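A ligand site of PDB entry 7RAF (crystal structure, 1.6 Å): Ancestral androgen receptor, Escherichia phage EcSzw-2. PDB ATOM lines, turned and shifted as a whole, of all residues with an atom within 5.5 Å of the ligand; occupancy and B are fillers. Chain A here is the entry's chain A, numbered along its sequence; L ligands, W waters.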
ATOM      1  N   LEU A  32     -13.020   5.622  -1.765  1.00  0.00           N
ATOM      2  CA  LEU A  32     -13.745   6.345  -2.816  1.00  0.00           C
ATOM      3  C   LEU A  32     -13.033   6.208  -4.162  1.00  0.00           C
ATOM      4  O   LEU A  32     -13.692   6.150  -5.190  1.00  0.00           O
ATOM      5  CB  LEU A  32     -13.900   7.816  -2.427  1.00  0.00           C
ATOM      6  CG  LEU A  32     -14.778   8.105  -1.199  1.00  0.00           C
ATOM      7  CD1 LEU A  32     -14.759   9.587  -0.877  1.00  0.00           C
ATOM      8  CD2 LEU A  32     -16.194   7.625  -1.425  1.00  0.00           C
ATOM      9  N   LEU A  35     -14.075   2.822  -5.519  1.00  0.00           N
ATOM     10  CA  LEU A  35     -15.430   2.884  -6.045  1.00  0.00           C
ATOM     11  C   LEU A  35     -15.474   3.580  -7.396  1.00  0.00           C
ATOM     12  O   LEU A  35     -16.210   3.143  -8.286  1.00  0.00           O
ATOM     13  CB  LEU A  35     -16.380   3.606  -5.084  1.00  0.00           C
ATOM     14  CG  LEU A  35     -16.719   2.863  -3.776  1.00  0.00           C
ATOM     15  CD1 LEU A  35     -17.505   3.834  -2.891  1.00  0.00           C
ATOM     16  CD2 LEU A  35     -17.564   1.616  -4.064  1.00  0.00           C
ATOM     17  N   ASN A  36     -14.702   4.657  -7.569  1.00  0.00           N
ATOM     18  CA  ASN A  36     -14.648   5.314  -8.881  1.00  0.00           C
ATOM     19  C   ASN A  36     -14.047   4.437  -9.971  1.00  0.00           C
ATOM     20  O   ASN A  36     -14.548   4.436 -11.089  1.00  0.00           O
ATOM     21  CB  ASN A  36     -13.847   6.606  -8.809  1.00  0.00           C
ATOM     22  CG  ASN A  36     -14.597   7.739  -8.233  1.00  0.00           C
ATOM     23  OD1 ASN A  36     -15.824   7.775  -8.221  1.00  0.00           O
ATOM     24  ND2 ASN A  36     -13.839   8.714  -7.761  1.00  0.00           N
ATOM     25  N   LEU A  38     -14.147   1.160  -9.996  1.00  0.00           N
ATOM     26  CA  LEU A  38     -15.206   0.191 -10.253  1.00  0.00           C
ATOM     27  C   LEU A  38     -16.321   0.801 -11.104  1.00  0.00           C
ATOM     28  O   LEU A  38     -16.817   0.151 -12.053  1.00  0.00           O
ATOM     29  CB  LEU A  38     -15.753  -0.271  -8.885  1.00  0.00           C
ATOM     30  CG  LEU A  38     -16.910  -1.236  -8.915  1.00  0.00           C
ATOM     31  CD1 LEU A  38     -16.491  -2.585  -9.561  1.00  0.00           C
ATOM     32  CD2 LEU A  38     -17.458  -1.441  -7.517  1.00  0.00           C
ATOM     33  N   GLY A  39     -16.728   2.027 -10.771  1.00  0.00           N
ATOM     34  CA  GLY A  39     -17.739   2.718 -11.541  1.00  0.00           C
ATOM     35  C   GLY A  39     -17.360   2.854 -13.001  1.00  0.00           C
ATOM     36  O   GLY A  39     -18.222   2.661 -13.890  1.00  0.00           O
ATOM     37  N   GLN A  42     -17.729  -0.524 -14.601  1.00  0.00           N
ATOM     38  CA  GLN A  42     -19.158  -0.838 -14.740  1.00  0.00           C
ATOM     39  C   GLN A  42     -19.774  -0.019 -15.865  1.00  0.00           C
ATOM     40  O   GLN A  42     -20.634  -0.512 -16.595  1.00  0.00           O
ATOM     41  CB  GLN A  42     -19.906  -0.594 -13.424  1.00  0.00           C
ATOM     42  CG  GLN A  42     -19.610  -1.662 -12.329  1.00  0.00           C
ATOM     43  CD  GLN A  42     -20.467  -1.441 -11.152  1.00  0.00           C
ATOM     44  OE1 GLN A  42     -21.424  -0.664 -11.208  1.00  0.00           O
ATOM     45  NE2 GLN A  42     -20.167  -2.135 -10.065  1.00  0.00           N
ATOM     46  N   TRP A  72     -26.812   6.445 -15.204  1.00  0.00           N
ATOM     47  CA  TRP A  72     -25.813   5.485 -14.731  1.00  0.00           C
ATOM     48  C   TRP A  72     -25.871   5.297 -13.232  1.00  0.00           C
ATOM     49  O   TRP A  72     -25.723   4.161 -12.746  1.00  0.00           O
ATOM     50  CB  TRP A  72     -24.395   5.901 -15.182  1.00  0.00           C
ATOM     51  CG  TRP A  72     -23.875   7.207 -14.673  1.00  0.00           C
ATOM     52  CD1 TRP A  72     -24.021   8.438 -15.269  1.00  0.00           C
ATOM     53  CD2 TRP A  72     -23.131   7.459 -13.454  1.00  0.00           C
ATOM     54  NE1 TRP A  72     -23.451   9.401 -14.488  1.00  0.00           N
ATOM     55  CE2 TRP A  72     -22.908   8.834 -13.371  1.00  0.00           C
ATOM     56  CE3 TRP A  72     -22.666   6.634 -12.412  1.00  0.00           C
ATOM     57  CZ2 TRP A  72     -22.190   9.428 -12.330  1.00  0.00           C
ATOM     58  CZ3 TRP A  72     -21.974   7.244 -11.367  1.00  0.00           C
ATOM     59  CH2 TRP A  72     -21.760   8.631 -11.330  1.00  0.00           C
ATOM     60  N   MET A  73     -26.077   6.369 -12.450  1.00  0.00           N
ATOM     61  CA  MET A  73     -26.051   6.212 -10.999  1.00  0.00           C
ATOM     62  C   MET A  73     -27.190   5.301 -10.531  1.00  0.00           C
ATOM     63  O   MET A  73     -26.972   4.377  -9.756  1.00  0.00           O
ATOM     64  CB  MET A  73     -26.150   7.562 -10.313  1.00  0.00           C
ATOM     65  CG  MET A  73     -26.166   7.511  -8.788  1.00  0.00           C
ATOM     66  SD  MET A  73     -24.538   7.121  -8.111  1.00  0.00           S
ATOM     67  CE  MET A  73     -23.777   8.737  -8.323  1.00  0.00           C
ATOM     68  N   MET A  76     -26.572   1.663 -11.573  1.00  0.00           N
ATOM     69  CA  MET A  76     -25.493   1.005 -10.817  1.00  0.00           C
ATOM     70  C   MET A  76     -25.877   0.823  -9.346  1.00  0.00           C
ATOM     71  O   MET A  76     -25.531  -0.206  -8.756  1.00  0.00           O
ATOM     72  CB  MET A  76     -24.189   1.774 -10.942  1.00  0.00           C
ATOM     73  CG  MET A  76     -23.653   1.640 -12.273  1.00  0.00           C
ATOM     74  SD  MET A  76     -22.101   2.682 -12.430  1.00  0.00           S
ATOM     75  CE  MET A  76     -22.102   2.551 -14.113  1.00  0.00           C
ATOM     76  N   VAL A  77     -26.580   1.779  -8.735  1.00  0.00           N
ATOM     77  CA  VAL A  77     -27.023   1.609  -7.348  1.00  0.00           C
ATOM     78  C   VAL A  77     -27.996   0.447  -7.254  1.00  0.00           C
ATOM     79  O   VAL A  77     -27.964  -0.373  -6.310  1.00  0.00           O
ATOM     80  CB  VAL A  77     -27.637   2.919  -6.810  1.00  0.00           C
ATOM     81  CG1 VAL A  77     -28.261   2.662  -5.474  1.00  0.00           C
ATOM     82  CG2 VAL A  77     -26.622   4.006  -6.665  1.00  0.00           C
ATOM     83  N   MET A  80     -26.263  -2.819  -7.584  1.00  0.00           N
ATOM     84  CA  MET A  80     -25.517  -3.117  -6.363  1.00  0.00           C
ATOM     85  C   MET A  80     -26.447  -3.584  -5.263  1.00  0.00           C
ATOM     86  O   MET A  80     -26.118  -4.536  -4.517  1.00  0.00           O
ATOM     87  CB  MET A  80     -24.733  -1.856  -5.956  1.00  0.00           C
ATOM     88  CG  MET A  80     -23.869  -1.982  -4.710  1.00  0.00           C
ATOM     89  SD  MET A  80     -24.692  -1.896  -3.162  1.00  0.00           S
ATOM     90  CE  MET A  80     -25.109  -0.141  -3.225  1.00  0.00           C
ATOM     91  N   ARG A  83     -27.082  -7.227  -5.994  1.00  0.00           N
ATOM     92  CA  ARG A  83     -25.950  -8.056  -5.600  1.00  0.00           C
ATOM     93  C   ARG A  83     -25.881  -8.209  -4.100  1.00  0.00           C
ATOM     94  O   ARG A  83     -25.498  -9.280  -3.601  1.00  0.00           O
ATOM     95  CB  ARG A  83     -24.623  -7.438  -6.089  1.00  0.00           C
ATOM     96  CG  ARG A  83     -24.470  -7.444  -7.578  1.00  0.00           C
ATOM     97  CD  ARG A  83     -23.019  -7.114  -7.958  1.00  0.00           C
ATOM     98  NE  ARG A  83     -22.626  -5.763  -7.606  1.00  0.00           N
ATOM     99  CZ  ARG A  83     -22.866  -4.661  -8.323  1.00  0.00           C
ATOM    100  NH1 ARG A  83     -23.560  -4.759  -9.440  1.00  0.00           N
ATOM    101  NH2 ARG A  83     -22.420  -3.486  -7.906  1.00  0.00           N
ATOM    102  N   PHE A  95     -20.465  -3.975  -3.443  1.00  0.00           N
ATOM    103  CA  PHE A  95     -20.132  -3.204  -4.618  1.00  0.00           C
ATOM    104  C   PHE A  95     -19.460  -4.105  -5.647  1.00  0.00           C
ATOM    105  O   PHE A  95     -19.762  -4.037  -6.865  1.00  0.00           O
ATOM    106  CB  PHE A  95     -19.229  -2.028  -4.253  1.00  0.00           C
ATOM    107  CG  PHE A  95     -19.886  -0.956  -3.505  1.00  0.00           C
ATOM    108  CD1 PHE A  95     -20.675  -0.042  -4.182  1.00  0.00           C
ATOM    109  CD2 PHE A  95     -19.708  -0.822  -2.131  1.00  0.00           C
ATOM    110  CE1 PHE A  95     -21.295   0.996  -3.502  1.00  0.00           C
ATOM    111  CE2 PHE A  95     -20.316   0.204  -1.439  1.00  0.00           C
ATOM    112  CZ  PHE A  95     -21.104   1.118  -2.133  1.00  0.00           C
ATOM    113  N   MET A 111     -19.283   8.852   3.419  1.00  0.00           N
ATOM    114  CA  MET A 111     -20.695   8.915   3.012  1.00  0.00           C
ATOM    115  C   MET A 111     -21.492   7.850   3.751  1.00  0.00           C
ATOM    116  O   MET A 111     -22.307   7.115   3.195  1.00  0.00           O
ATOM    117  CB  MET A 111     -20.876   8.801   1.493  1.00  0.00           C
ATOM    118  CG  MET A 111     -20.247   7.687   0.946  1.00  0.00           C
ATOM    119  SD  MET A 111     -20.968   7.423  -0.787  1.00  0.00           S
ATOM    120  CE  MET A 111     -19.928   6.122  -1.157  1.00  0.00           C
ATOM    121  N   MET A 118     -28.383   3.164   0.940  1.00  0.00           N
ATOM    122  CA  MET A 118     -28.211   2.118  -0.069  1.00  0.00           C
ATOM    123  C   MET A 118     -28.446   0.738   0.517  1.00  0.00           C
ATOM    124  O   MET A 118     -28.961  -0.136  -0.179  1.00  0.00           O
ATOM    125  CB  MET A 118     -26.816   2.204  -0.749  1.00  0.00           C
ATOM    126  CG  MET A 118     -26.687   3.449  -1.665  1.00  0.00           C
ATOM    127  SD  MET A 118     -25.165   3.494  -2.616  1.00  0.00           S
ATOM    128  CE  MET A 118     -24.023   4.060  -1.426  1.00  0.00           C
ATOM    129  N   LEU A 204     -27.036  11.073  -3.955  1.00  0.00           N
ATOM    130  CA  LEU A 204     -25.751  10.550  -4.435  1.00  0.00           C
ATOM    131  C   LEU A 204     -25.125  11.492  -5.467  1.00  0.00           C
ATOM    132  O   LEU A 204     -23.901  11.667  -5.473  1.00  0.00           O
ATOM    133  CB  LEU A 204     -25.951   9.141  -5.004  1.00  0.00           C
ATOM    134  CG  LEU A 204     -26.238   8.073  -3.955  1.00  0.00           C
ATOM    135  CD1 LEU A 204     -26.788   6.837  -4.667  1.00  0.00           C
ATOM    136  CD2 LEU A 204     -25.002   7.694  -3.143  1.00  0.00           C
ATOM    137  N   PHE A 207     -23.423  14.316  -3.559  1.00  0.00           N
ATOM    138  CA  PHE A 207     -22.170  13.903  -2.959  1.00  0.00           C
ATOM    139  C   PHE A 207     -21.105  13.689  -4.022  1.00  0.00           C
ATOM    140  O   PHE A 207     -19.933  14.043  -3.809  1.00  0.00           O
ATOM    141  CB  PHE A 207     -22.357  12.640  -2.138  1.00  0.00           C
ATOM    142  CG  PHE A 207     -21.142  12.233  -1.350  1.00  0.00           C
ATOM    143  CD1 PHE A 207     -20.194  11.382  -1.919  1.00  0.00           C
ATOM    144  CD2 PHE A 207     -20.944  12.629  -0.025  1.00  0.00           C
ATOM    145  CE1 PHE A 207     -19.100  11.029  -1.200  1.00  0.00           C
ATOM    146  CE2 PHE A 207     -19.816  12.233   0.672  1.00  0.00           C
ATOM    147  CZ  PHE A 207     -18.909  11.444   0.066  1.00  0.00           C
ATOM    148  N   THR A 208     -21.488  13.149  -5.184  1.00  0.00           N
ATOM    149  CA  THR A 208     -20.568  12.961  -6.288  1.00  0.00           C
ATOM    150  C   THR A 208     -19.997  14.310  -6.713  1.00  0.00           C
ATOM    151  O   THR A 208     -18.780  14.445  -6.950  1.00  0.00           O
ATOM    152  CB  THR A 208     -21.275  12.294  -7.473  1.00  0.00           C
ATOM    153  OG1 THR A 208     -21.741  11.010  -7.048  1.00  0.00           O
ATOM    154  CG2 THR A 208     -20.365  12.059  -8.613  1.00  0.00           C
ATOM    155  N   THR A 211     -17.520  15.651  -4.196  1.00  0.00           N
ATOM    156  CA  THR A 211     -16.258  14.905  -4.187  1.00  0.00           C
ATOM    157  C   THR A 211     -15.467  15.230  -5.446  1.00  0.00           C
ATOM    158  O   THR A 211     -14.241  15.429  -5.381  1.00  0.00           O
ATOM    159  CB  THR A 211     -16.532  13.401  -4.083  1.00  0.00           C
ATOM    160  OG1 THR A 211     -17.348  13.156  -2.924  1.00  0.00           O
ATOM    161  CG2 THR A 211     -15.270  12.605  -3.908  1.00  0.00           C
ATOM    162  N   VAL A 220      -8.847  11.871  -4.213  1.00  0.00           N
ATOM    163  CA  VAL A 220      -9.804  10.950  -4.799  1.00  0.00           C
ATOM    164  C   VAL A 220      -9.800  11.159  -6.295  1.00  0.00           C
ATOM    165  O   VAL A 220     -10.371  12.127  -6.804  1.00  0.00           O
ATOM    166  CB  VAL A 220     -11.215  11.145  -4.235  1.00  0.00           C
ATOM    167  CG1 VAL A 220     -12.242  10.292  -4.992  1.00  0.00           C
ATOM    168  CG2 VAL A 220     -11.258  10.845  -2.741  1.00  0.00           C
ATOM    169  N   PHE A 222     -10.820  10.524 -10.150  1.00  0.00           N
ATOM    170  CA  PHE A 222     -11.930  10.116 -11.001  1.00  0.00           C
ATOM    171  C   PHE A 222     -11.370   9.702 -12.357  1.00  0.00           C
ATOM    172  O   PHE A 222     -10.722  10.513 -13.053  1.00  0.00           O
ATOM    173  CB  PHE A 222     -12.942  11.222 -11.191  1.00  0.00           C
ATOM    174  CG  PHE A 222     -13.785  11.469 -10.001  1.00  0.00           C
ATOM    175  CD1 PHE A 222     -13.279  12.211  -8.924  1.00  0.00           C
ATOM    176  CD2 PHE A 222     -15.064  10.978  -9.949  1.00  0.00           C
ATOM    177  CE1 PHE A 222     -14.077  12.448  -7.837  1.00  0.00           C
ATOM    178  CE2 PHE A 222     -15.889  11.200  -8.833  1.00  0.00           C
ATOM    179  CZ  PHE A 222     -15.398  11.930  -7.804  1.00  0.00           C
ATOM    180  N   MET A 226     -15.745   8.547 -16.213  1.00  0.00           N
ATOM    181  CA  MET A 226     -16.538   9.086 -15.106  1.00  0.00           C
ATOM    182  C   MET A 226     -16.426  10.599 -15.004  1.00  0.00           C
ATOM    183  O   MET A 226     -17.431  11.299 -14.809  1.00  0.00           O
ATOM    184  CB  MET A 226     -16.143   8.442 -13.760  1.00  0.00           C
ATOM    185  CG  MET A 226     -16.943   7.220 -13.352  1.00  0.00           C
ATOM    186  SD  MET A 226     -16.569   7.022 -11.611  1.00  0.00           S
ATOM    187  CE  MET A 226     -18.015   7.708 -10.860  1.00  0.00           C
HETATM  188  C1  LIG L   1     -19.722   2.361  -7.963  1.00  0.00           C
HETATM  189  C2  LIG L   1     -20.275   1.118  -8.646  1.00  0.00           C
HETATM  190  C3  LIG L   1     -21.361   0.575  -7.890  1.00  0.00           C
HETATM  191  O1  LIG L   1     -21.547  -0.611  -7.728  1.00  0.00           O
HETATM  192  C4  LIG L   1     -22.265   1.462  -7.145  1.00  0.00           C
HETATM  193  C5  LIG L   1     -21.983   2.963  -7.144  1.00  0.00           C
HETATM  194  C6  LIG L   1     -22.976   3.787  -6.543  1.00  0.00           C
HETATM  195  C7  LIG L   1     -22.234   5.025  -5.705  1.00  0.00           C
HETATM  196  C8  LIG L   1     -21.261   5.618  -6.276  1.00  0.00           C
HETATM  197  C9  LIG L   1     -20.254   4.623  -6.739  1.00  0.00           C
HETATM  198  C10 LIG L   1     -20.840   3.478  -7.713  1.00  0.00           C
HETATM  199  C11 LIG L   1     -18.973   5.301  -7.311  1.00  0.00           C
HETATM  200  C12 LIG L   1     -18.479   6.272  -6.551  1.00  0.00           C
HETATM  201  C13 LIG L   1     -19.409   7.223  -6.119  1.00  0.00           C
HETATM  202  C14 LIG L   1     -20.759   6.400  -5.656  1.00  0.00           C
HETATM  203  C15 LIG L   1     -21.606   7.669  -4.911  1.00  0.00           C
HETATM  204  C16 LIG L   1     -20.474   8.879  -4.406  1.00  0.00           C
HETATM  205  C17 LIG L   1     -19.041   8.317  -4.845  1.00  0.00           C
HETATM  206  C18 LIG L   1     -19.822   8.163  -7.296  1.00  0.00           C
HETATM  207  C19 LIG L   1     -21.230   4.049  -9.082  1.00  0.00           C
HETATM  208  C20 LIG L   1     -18.113   9.289  -5.161  1.00  0.00           C
HETATM  209  O2  LIG L   1     -18.378  10.469  -5.266  1.00  0.00           O
HETATM  210  C21 LIG L   1     -16.643   8.974  -5.348  1.00  0.00           C
HETATM  211  O   HOH W   1     -23.613  -1.785  -9.997  1.00  0.00           O
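NH2 of Arg 83 is in hydrogen-bond range of O1 of the ligand.
The side-chain amide nitrogen of Gln 42 lies within hydrogen-bond range of an oxygen (O1) of the ligand (3.1 Å).
Leu 35 touches the ligand.
Asn 36 touches the ligand (OD1 to C21, 3.2 Å).
CD2 of Leu 38 touches C2 of the ligand, 3.97 Å away.
CZ3 of Trp 72 touches C19 of the ligand (3.998 Å).
SD of Met 73 touches C7 of the ligand, 3.9 Å away.
Met 76 touches the ligand.
Val 77 touches the ligand.
CB of Met 80 touches O1 of the ligand, 3.9 Å away.
Phe 95 touches the ligand (CD1 to C4, 3.7 Å).
Met 111 touches the ligand (SD to C16, 3.9 Å).
Leu 204 touches the ligand (CD2 to C15, 3.8 Å).
Phe 207 touches the ligand (CD1 to C16, 3.5 Å).
OG1 of Thr 208 touches C18 of the ligand, 3.4 Å away.
Thr 211 touches the ligand (CB to O2, 3.7 Å).
Hydrophobic or aromatic side chains within 4 Å of the ligand: Leu 35, Leu 38, Trp 72, Met 73, Met 76, Val 77, Met 80, Phe 95, Met 111, Leu 204 and Phe 207.
NH2 of Arg 83 lies close to NE2 of Gln 42 (3.4 Å).
The backbone carbonyl oxygen (O) of Phe 95 lies within hydrogen-bond range of the guanidinium group (NH2) of Arg 83 (2.9 Å).
The side-chain amide oxygen (OE1) of Gln 42 lies close to the side-chain sulfur (SD) of Met 76 (3.6 Å).
The side-chain amide oxygen (OD1) of Asn 36 lies close to the side-chain sulfur (SD) of Met 226 (3.6 Å).
OG1 of Thr 208 lies within hydrogen-bond range of O of Leu 204, at 2.8 Å.
The backbone carbonyl oxygen (O) of Phe 207 sits at hydrogen-bond distance from the side-chain hydroxyl (OG1) of Thr 211 (2.9 Å).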
